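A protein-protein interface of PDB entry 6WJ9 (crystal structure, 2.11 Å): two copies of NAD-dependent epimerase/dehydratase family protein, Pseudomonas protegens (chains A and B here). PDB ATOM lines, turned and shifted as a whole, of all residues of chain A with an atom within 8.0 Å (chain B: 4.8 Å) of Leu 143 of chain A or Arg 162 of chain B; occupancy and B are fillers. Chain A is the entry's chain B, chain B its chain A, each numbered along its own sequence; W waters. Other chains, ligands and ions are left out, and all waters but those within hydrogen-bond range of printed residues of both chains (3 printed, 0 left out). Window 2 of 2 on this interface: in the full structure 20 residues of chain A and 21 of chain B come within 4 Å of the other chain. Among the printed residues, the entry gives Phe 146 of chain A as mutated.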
ATOM      1  N   VAL A  83     -13.711   3.209   6.324  1.00  0.00           N
ATOM      2  CA  VAL A  83     -14.823   2.336   5.949  1.00  0.00           C
ATOM      3  C   VAL A  83     -15.840   3.077   5.080  1.00  0.00           C
ATOM      4  O   VAL A  83     -16.341   2.530   4.087  1.00  0.00           O
ATOM      5  CB  VAL A  83     -15.479   1.752   7.216  1.00  0.00           C
ATOM      6  CG1 VAL A  83     -16.734   0.979   6.863  1.00  0.00           C
ATOM      7  CG2 VAL A  83     -14.496   0.855   7.960  1.00  0.00           C
ATOM      8  N   SER A  86     -15.395   3.063   1.445  1.00  0.00           N
ATOM      9  CA  SER A  86     -15.729   1.839   0.725  1.00  0.00           C
ATOM     10  C   SER A  86     -17.231   1.698   0.531  1.00  0.00           C
ATOM     11  O   SER A  86     -17.672   1.041  -0.417  1.00  0.00           O
ATOM     12  CB  SER A  86     -15.171   0.622   1.458  1.00  0.00           C
ATOM     13  OG  SER A  86     -16.031   0.235   2.510  1.00  0.00           O
ATOM     14  N   VAL A  87     -18.028   2.304   1.414  1.00  0.00           N
ATOM     15  CA  VAL A  87     -19.472   2.289   1.231  1.00  0.00           C
ATOM     16  C   VAL A  87     -19.857   3.185   0.066  1.00  0.00           C
ATOM     17  O   VAL A  87     -20.753   2.855  -0.720  1.00  0.00           O
ATOM     18  CB  VAL A  87     -20.173   2.702   2.539  1.00  0.00           C
ATOM     19  CG1 VAL A  87     -21.669   2.924   2.313  1.00  0.00           C
ATOM     20  CG2 VAL A  87     -19.950   1.631   3.608  1.00  0.00           C
ATOM     21  N   ALA A 123     -13.098  -5.008  12.007  1.00  0.00           N
ATOM     22  CA  ALA A 123     -14.315  -4.927  11.205  1.00  0.00           C
ATOM     23  C   ALA A 123     -14.769  -6.285  10.647  1.00  0.00           C
ATOM     24  O   ALA A 123     -15.957  -6.446  10.347  1.00  0.00           O
ATOM     25  CB  ALA A 123     -14.100  -3.925  10.065  1.00  0.00           C
ATOM     26  N   VAL A 124     -13.876  -7.272  10.518  1.00  0.00           N
ATOM     27  CA  VAL A 124     -14.298  -8.574   9.967  1.00  0.00           C
ATOM     28  C   VAL A 124     -15.332  -9.267  10.855  1.00  0.00           C
ATOM     29  O   VAL A 124     -16.077 -10.130  10.372  1.00  0.00           O
ATOM     30  CB  VAL A 124     -13.096  -9.524   9.732  1.00  0.00           C
ATOM     31  CG1 VAL A 124     -12.055  -8.898   8.788  1.00  0.00           C
ATOM     32  CG2 VAL A 124     -12.454  -9.930  11.048  1.00  0.00           C
ATOM     33  N   TYR A 125     -15.402  -8.904  12.142  1.00  0.00           N
ATOM     34  CA  TYR A 125     -16.369  -9.501  13.061  1.00  0.00           C
ATOM     35  C   TYR A 125     -17.751  -8.878  12.956  1.00  0.00           C
ATOM     36  O   TYR A 125     -18.724  -9.489  13.414  1.00  0.00           O
ATOM     37  CB  TYR A 125     -15.897  -9.366  14.522  1.00  0.00           C
ATOM     38  CG  TYR A 125     -14.546  -9.978  14.802  1.00  0.00           C
ATOM     39  CD1 TYR A 125     -14.341 -11.345  14.680  1.00  0.00           C
ATOM     40  CD2 TYR A 125     -13.474  -9.189  15.197  1.00  0.00           C
ATOM     41  CE1 TYR A 125     -13.102 -11.913  14.944  1.00  0.00           C
ATOM     42  CE2 TYR A 125     -12.231  -9.745  15.464  1.00  0.00           C
ATOM     43  CZ  TYR A 125     -12.052 -11.106  15.334  1.00  0.00           C
ATOM     44  OH  TYR A 125     -10.817 -11.662  15.596  1.00  0.00           O
ATOM     45  N   GLY A 126     -17.860  -7.679  12.388  1.00  0.00           N
ATOM     46  CA  GLY A 126     -19.141  -6.985  12.420  1.00  0.00           C
ATOM     47  C   GLY A 126     -19.623  -6.822  13.855  1.00  0.00           C
ATOM     48  O   GLY A 126     -18.853  -6.473  14.761  1.00  0.00           O
ATOM     49  N   ASN A 127     -20.905  -7.112  14.076  1.00  0.00           N
ATOM     50  CA  ASN A 127     -21.512  -7.059  15.401  1.00  0.00           C
ATOM     51  C   ASN A 127     -21.391  -8.357  16.196  1.00  0.00           C
ATOM     52  O   ASN A 127     -21.920  -8.422  17.315  1.00  0.00           O
ATOM     53  CB  ASN A 127     -22.994  -6.691  15.282  1.00  0.00           C
ATOM     54  CG  ASN A 127     -23.214  -5.203  15.201  1.00  0.00           C
ATOM     55  OD1 ASN A 127     -23.604  -4.566  16.185  1.00  0.00           O
ATOM     56  ND2 ASN A 127     -22.962  -4.632  14.029  1.00  0.00           N
ATOM     57  N   ASN A 128     -20.745  -9.395  15.656  1.00  0.00           N
ATOM     58  CA  ASN A 128     -20.658 -10.663  16.377  1.00  0.00           C
ATOM     59  C   ASN A 128     -19.725 -10.531  17.574  1.00  0.00           C
ATOM     60  O   ASN A 128     -18.598 -10.044  17.451  1.00  0.00           O
ATOM     61  CB  ASN A 128     -20.180 -11.784  15.456  1.00  0.00           C
ATOM     62  CG  ASN A 128     -21.229 -12.174  14.440  1.00  0.00           C
ATOM     63  OD1 ASN A 128     -22.410 -11.899  14.631  1.00  0.00           O
ATOM     64  ND2 ASN A 128     -20.802 -12.786  13.339  1.00  0.00           N
ATOM     65  N   LYS A 140     -17.463 -14.621  11.498  1.00  0.00           N
ATOM     66  CA  LYS A 140     -17.227 -13.352  10.822  1.00  0.00           C
ATOM     67  C   LYS A 140     -18.528 -12.767  10.291  1.00  0.00           C
ATOM     68  O   LYS A 140     -19.465 -13.494   9.955  1.00  0.00           O
ATOM     69  CB  LYS A 140     -16.234 -13.550   9.681  1.00  0.00           C
ATOM     70  CG  LYS A 140     -14.941 -14.244  10.119  1.00  0.00           C
ATOM     71  CD  LYS A 140     -14.251 -13.451  11.236  1.00  0.00           C
ATOM     72  CE  LYS A 140     -13.030 -14.194  11.759  1.00  0.00           C
ATOM     73  NZ  LYS A 140     -13.403 -15.545  12.319  1.00  0.00           N
ATOM     74  N   SER A 141     -18.589 -11.434  10.216  1.00  0.00           N
ATOM     75  CA  SER A 141     -19.759 -10.745   9.666  1.00  0.00           C
ATOM     76  C   SER A 141     -19.349  -9.390   9.111  1.00  0.00           C
ATOM     77  O   SER A 141     -19.768  -8.340   9.612  1.00  0.00           O
ATOM     78  CB  SER A 141     -20.840 -10.603  10.736  1.00  0.00           C
ATOM     79  OG  SER A 141     -22.014 -10.048  10.190  1.00  0.00           O
ATOM     80  N   PRO A 142     -18.516  -9.371   8.065  1.00  0.00           N
ATOM     81  CA  PRO A 142     -18.129  -8.084   7.462  1.00  0.00           C
ATOM     82  C   PRO A 142     -19.337  -7.392   6.849  1.00  0.00           C
ATOM     83  O   PRO A 142     -20.039  -7.958   6.010  1.00  0.00           O
ATOM     84  CB  PRO A 142     -17.092  -8.488   6.407  1.00  0.00           C
ATOM     85  CG  PRO A 142     -17.404  -9.923   6.099  1.00  0.00           C
ATOM     86  CD  PRO A 142     -17.916 -10.521   7.363  1.00  0.00           C
ATOM     87  N   LEU A 143     -19.580  -6.147   7.277  1.00  0.00           N
ATOM     88  CA  LEU A 143     -20.788  -5.413   6.895  1.00  0.00           C
ATOM     89  C   LEU A 143     -20.573  -4.400   5.776  1.00  0.00           C
ATOM     90  O   LEU A 143     -21.557  -3.878   5.247  1.00  0.00           O
ATOM     91  CB  LEU A 143     -21.374  -4.679   8.120  1.00  0.00           C
ATOM     92  CG  LEU A 143     -21.829  -5.564   9.286  1.00  0.00           C
ATOM     93  CD1 LEU A 143     -22.128  -4.710  10.527  1.00  0.00           C
ATOM     94  CD2 LEU A 143     -23.065  -6.405   8.892  1.00  0.00           C
ATOM     95  N   THR A 144     -19.334  -4.116   5.402  1.00  0.00           N
ATOM     96  CA  THR A 144     -18.997  -3.131   4.383  1.00  0.00           C
ATOM     97  C   THR A 144     -18.005  -3.745   3.407  1.00  0.00           C
ATOM     98  O   THR A 144     -17.376  -4.758   3.716  1.00  0.00           O
ATOM     99  CB  THR A 144     -18.373  -1.882   5.020  1.00  0.00           C
ATOM    100  OG1 THR A 144     -17.213  -2.274   5.769  1.00  0.00           O
ATOM    101  CG2 THR A 144     -19.390  -1.181   5.941  1.00  0.00           C
ATOM    102  N   PRO A 145     -17.845  -3.144   2.216  1.00  0.00           N
ATOM    103  CA  PRO A 145     -16.798  -3.633   1.297  1.00  0.00           C
ATOM    104  C   PRO A 145     -15.404  -3.634   1.908  1.00  0.00           C
ATOM    105  O   PRO A 145     -14.644  -4.579   1.666  1.00  0.00           O
ATOM    106  CB  PRO A 145     -16.903  -2.668   0.104  1.00  0.00           C
ATOM    107  CG  PRO A 145     -18.334  -2.221   0.117  1.00  0.00           C
ATOM    108  CD  PRO A 145     -18.709  -2.132   1.578  1.00  0.00           C
ATOM    109  N   PHE A 146     -15.043  -2.606   2.688  1.00  0.00           N
ATOM    110  CA  PHE A 146     -13.758  -2.625   3.390  1.00  0.00           C
ATOM    111  C   PHE A 146     -13.610  -3.895   4.225  1.00  0.00           C
ATOM    112  O   PHE A 146     -12.615  -4.615   4.115  1.00  0.00           O
ATOM    113  CB  PHE A 146     -13.610  -1.374   4.280  1.00  0.00           C
ATOM    114  CG  PHE A 146     -12.442  -1.437   5.246  1.00  0.00           C
ATOM    115  CD1 PHE A 146     -11.175  -1.030   4.850  1.00  0.00           C
ATOM    116  CD2 PHE A 146     -12.616  -1.887   6.550  1.00  0.00           C
ATOM    117  CE1 PHE A 146     -10.091  -1.080   5.734  1.00  0.00           C
ATOM    118  CE2 PHE A 146     -11.539  -1.951   7.442  1.00  0.00           C
ATOM    119  CZ  PHE A 146     -10.267  -1.549   7.027  1.00  0.00           C
ATOM    120  N   ALA A 147     -14.597  -4.185   5.063  1.00  0.00           N
ATOM    121  CA  ALA A 147     -14.461  -5.317   5.974  1.00  0.00           C
ATOM    122  C   ALA A 147     -14.420  -6.632   5.212  1.00  0.00           C
ATOM    123  O   ALA A 147     -13.658  -7.538   5.565  1.00  0.00           O
ATOM    124  CB  ALA A 147     -15.612  -5.323   6.988  1.00  0.00           C
ATOM    125  N   ALA A 148     -15.255  -6.764   4.183  1.00  0.00           N
ATOM    126  CA  ALA A 148     -15.233  -7.976   3.373  1.00  0.00           C
ATOM    127  C   ALA A 148     -13.906  -8.133   2.644  1.00  0.00           C
ATOM    128  O   ALA A 148     -13.421  -9.263   2.461  1.00  0.00           O
ATOM    129  CB  ALA A 148     -16.402  -7.945   2.388  1.00  0.00           C
ATOM    130  N   GLY A 275     -24.464   3.273  12.019  1.00  0.00           N
ATOM    131  CA  GLY A 275     -23.826   1.967  12.067  1.00  0.00           C
ATOM    132  C   GLY A 275     -23.122   1.621  13.362  1.00  0.00           C
ATOM    133  O   GLY A 275     -22.588   0.517  13.495  1.00  0.00           O
ATOM    134  N   ILE A 277     -21.239   0.542  16.458  1.00  0.00           N
ATOM    135  CA  ILE A 277     -21.164  -0.545  17.427  1.00  0.00           C
ATOM    136  C   ILE A 277     -20.851   0.050  18.790  1.00  0.00           C
ATOM    137  O   ILE A 277     -19.927   0.860  18.930  1.00  0.00           O
ATOM    138  CB  ILE A 277     -20.106  -1.577  17.008  1.00  0.00           C
ATOM    139  CG1 ILE A 277     -20.504  -2.216  15.678  1.00  0.00           C
ATOM    140  CG2 ILE A 277     -19.942  -2.643  18.083  1.00  0.00           C
ATOM    141  CD1 ILE A 277     -19.454  -3.137  15.094  1.00  0.00           C
ATOM    142  N   ASP B 158     -25.037  -9.026   0.507  1.00  0.00           N
ATOM    143  CA  ASP B 158     -25.709  -8.603   1.734  1.00  0.00           C
ATOM    144  C   ASP B 158     -25.548  -7.101   1.975  1.00  0.00           C
ATOM    145  O   ASP B 158     -26.480  -6.436   2.451  1.00  0.00           O
ATOM    146  CB  ASP B 158     -25.175  -9.391   2.932  1.00  0.00           C
ATOM    147  CG  ASP B 158     -25.927  -9.060   4.214  1.00  0.00           C
ATOM    148  OD1 ASP B 158     -27.104  -9.455   4.326  1.00  0.00           O
ATOM    149  OD2 ASP B 158     -25.363  -8.364   5.080  1.00  0.00           O
ATOM    150  N   PHE B 159     -24.362  -6.554   1.683  1.00  0.00           N
ATOM    151  CA  PHE B 159     -24.177  -5.108   1.784  1.00  0.00           C
ATOM    152  C   PHE B 159     -25.111  -4.352   0.838  1.00  0.00           C
ATOM    153  O   PHE B 159     -25.695  -3.329   1.218  1.00  0.00           O
ATOM    154  CB  PHE B 159     -22.716  -4.744   1.511  1.00  0.00           C
ATOM    155  CG  PHE B 159     -22.499  -3.289   1.204  1.00  0.00           C
ATOM    156  CD1 PHE B 159     -22.526  -2.338   2.216  1.00  0.00           C
ATOM    157  CD2 PHE B 159     -22.261  -2.873  -0.096  1.00  0.00           C
ATOM    158  CE1 PHE B 159     -22.332  -0.989   1.929  1.00  0.00           C
ATOM    159  CE2 PHE B 159     -22.073  -1.525  -0.392  1.00  0.00           C
ATOM    160  CZ  PHE B 159     -22.100  -0.584   0.625  1.00  0.00           C
ATOM    161  N   TYR B 160     -25.272  -4.826  -0.402  1.00  0.00           N
ATOM    162  CA  TYR B 160     -26.190  -4.116  -1.296  1.00  0.00           C
ATOM    163  C   TYR B 160     -27.640  -4.256  -0.838  1.00  0.00           C
ATOM    164  O   TYR B 160     -28.443  -3.336  -1.040  1.00  0.00           O
ATOM    165  CB  TYR B 160     -26.014  -4.600  -2.739  1.00  0.00           C
ATOM    166  CG  TYR B 160     -24.868  -3.894  -3.444  1.00  0.00           C
ATOM    167  CD1 TYR B 160     -23.554  -4.324  -3.278  1.00  0.00           C
ATOM    168  CD2 TYR B 160     -25.101  -2.788  -4.260  1.00  0.00           C
ATOM    169  CE1 TYR B 160     -22.505  -3.680  -3.913  1.00  0.00           C
ATOM    170  CE2 TYR B 160     -24.054  -2.131  -4.898  1.00  0.00           C
ATOM    171  CZ  TYR B 160     -22.759  -2.580  -4.717  1.00  0.00           C
ATOM    172  OH  TYR B 160     -21.717  -1.934  -5.340  1.00  0.00           O
ATOM    173  N   ARG B 161     -27.986  -5.371  -0.189  1.00  0.00           N
ATOM    174  CA  ARG B 161     -29.315  -5.495   0.404  1.00  0.00           C
ATOM    175  C   ARG B 161     -29.562  -4.393   1.433  1.00  0.00           C
ATOM    176  O   ARG B 161     -30.533  -3.634   1.332  1.00  0.00           O
ATOM    177  CB  ARG B 161     -29.487  -6.874   1.050  1.00  0.00           C
ATOM    178  CG  ARG B 161     -30.824  -7.006   1.826  1.00  0.00           C
ATOM    179  CD  ARG B 161     -30.928  -8.357   2.546  1.00  0.00           C
ATOM    180  NE  ARG B 161     -29.904  -8.513   3.576  1.00  0.00           N
ATOM    181  CZ  ARG B 161     -30.006  -8.050   4.823  1.00  0.00           C
ATOM    182  NH1 ARG B 161     -31.093  -7.392   5.213  1.00  0.00           N
ATOM    183  NH2 ARG B 161     -29.019  -8.251   5.686  1.00  0.00           N
ATOM    184  N   ARG B 162     -28.676  -4.288   2.429  1.00  0.00           N
ATOM    185  CA  ARG B 162     -28.884  -3.333   3.513  1.00  0.00           C
ATOM    186  C   ARG B 162     -28.689  -1.900   3.032  1.00  0.00           C
ATOM    187  O   ARG B 162     -29.413  -0.997   3.461  1.00  0.00           O
ATOM    188  CB  ARG B 162     -27.932  -3.640   4.673  1.00  0.00           C
ATOM    189  CG  ARG B 162     -28.310  -4.871   5.491  1.00  0.00           C
ATOM    190  CD  ARG B 162     -27.236  -5.216   6.537  1.00  0.00           C
ATOM    191  NE  ARG B 162     -26.051  -5.793   5.914  1.00  0.00           N
ATOM    192  CZ  ARG B 162     -24.886  -5.162   5.787  1.00  0.00           C
ATOM    193  NH1 ARG B 162     -23.870  -5.757   5.187  1.00  0.00           N
ATOM    194  NH2 ARG B 162     -24.733  -3.939   6.265  1.00  0.00           N
ATOM    195  N   GLN B 163     -27.720  -1.666   2.146  1.00  0.00           N
ATOM    196  CA  GLN B 163     -27.386  -0.298   1.761  1.00  0.00           C
ATOM    197  C   GLN B 163     -28.195   0.207   0.570  1.00  0.00           C
ATOM    198  O   GLN B 163     -28.505   1.401   0.512  1.00  0.00           O
ATOM    199  CB  GLN B 163     -25.887  -0.185   1.458  1.00  0.00           C
ATOM    200  CG  GLN B 163     -25.386   1.238   1.188  1.00  0.00           C
ATOM    201  CD  GLN B 163     -25.349   2.115   2.434  1.00  0.00           C
ATOM    202  OE1 GLN B 163     -24.983   1.668   3.516  1.00  0.00           O
ATOM    203  NE2 GLN B 163     -25.722   3.367   2.276  1.00  0.00           N
ATOM    204  N   HIS B 164     -28.579  -0.664  -0.368  1.00  0.00           N
ATOM    205  CA  HIS B 164     -29.222  -0.200  -1.594  1.00  0.00           C
ATOM    206  C   HIS B 164     -30.489  -0.985  -1.939  1.00  0.00           C
ATOM    207  O   HIS B 164     -30.969  -0.901  -3.072  1.00  0.00           O
ATOM    208  CB  HIS B 164     -28.237  -0.253  -2.762  1.00  0.00           C
ATOM    209  CG  HIS B 164     -26.998   0.556  -2.540  1.00  0.00           C
ATOM    210  ND1 HIS B 164     -26.998   1.936  -2.542  1.00  0.00           N
ATOM    211  CD2 HIS B 164     -25.718   0.181  -2.308  1.00  0.00           C
ATOM    212  CE1 HIS B 164     -25.772   2.375  -2.321  1.00  0.00           C
ATOM    213  NE2 HIS B 164     -24.975   1.329  -2.172  1.00  0.00           N
ATOM    214  N   GLY B 165     -31.042  -1.745  -1.000  1.00  0.00           N
ATOM    215  CA  GLY B 165     -32.348  -2.348  -1.213  1.00  0.00           C
ATOM    216  C   GLY B 165     -32.385  -3.562  -2.119  1.00  0.00           C
ATOM    217  O   GLY B 165     -33.482  -3.996  -2.492  1.00  0.00           O
HETATM  218  O   HOH W   1     -22.348   1.425  -2.565  1.00  0.00           O
HETATM  219  O   HOH W   2     -22.819  -1.631   6.276  1.00  0.00           O
HETATM  220  O   HOH W   3     -21.781  -7.276   4.075  1.00  0.00           O
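Water W1 lies within hydrogen-bond range of a ring nitrogen (NE2) of His 164 of chain B (2.7 Å) and the backbone carbonyl oxygen of Val 87 of chain A (2.8 Å).
Water W3 lies within hydrogen-bond range of O of Pro 142 of chain A (2.7 Å) and NH1 of Arg 162 of chain B (2.8 Å).
Water W2 bridges O of Leu 143 of chain A (2.8 Å) and NH2 of Arg 162 of chain B (3.0 Å).
Val 87 of chain A touches Phe 159 of chain B.
Gln 163 of chain B touches Val 87 of chain A.
Phe 159 of chain B touches Leu 143 of chain A (CD1 to O, 3.5 Å).
Pro 145 of chain A touches Phe 159 of chain B (CD to CE1, 3.8 Å).
Of the printed residues of chain B, Val 87 of chain A touches Phe 159 and Gln 163.
Of the printed residues of chain B, Leu 143 of chain A touches Phe 159 and Arg 162.
Printed residues of chain B within 4 Å of Pro 145 of chain A: Phe 159 (3.8 Å).
Arg 162 of chain B touches just one residue of chain A: Leu 143.
Printed residues of chain A within 4 Å of Gln 163 of chain B: Val 87.
The guanidinium group of Arg 162 of chain B lies within hydrogen-bond range of the backbone carbonyl oxygen of Leu 143 of chain A (3.0 Å).
Of the 20 printed residues of chain A, 3 touch a printed residue of chain B.
Hydrophobic or aromatic side chains of chain A that line the printed part of chain B: Val 87, Leu 143 and Pro 145.
Of the 8 printed residues of chain B, 3 touch a printed residue of chain A.
Among the printed residues, no Asp or Glu carboxylate lies within 4 Å of a Lys or Arg side-chain nitrogen of the other chain.
No position is printed for both chains.
Of the 5 pairs that touch across the chains among the printed residues, none has its exchanged pair printed and touching as well.
The side-chain carboxylate of Asp 158 of chain B is in salt-bridge range of the guanidinium group of Arg 162 of chain B, 2.8 Å away.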
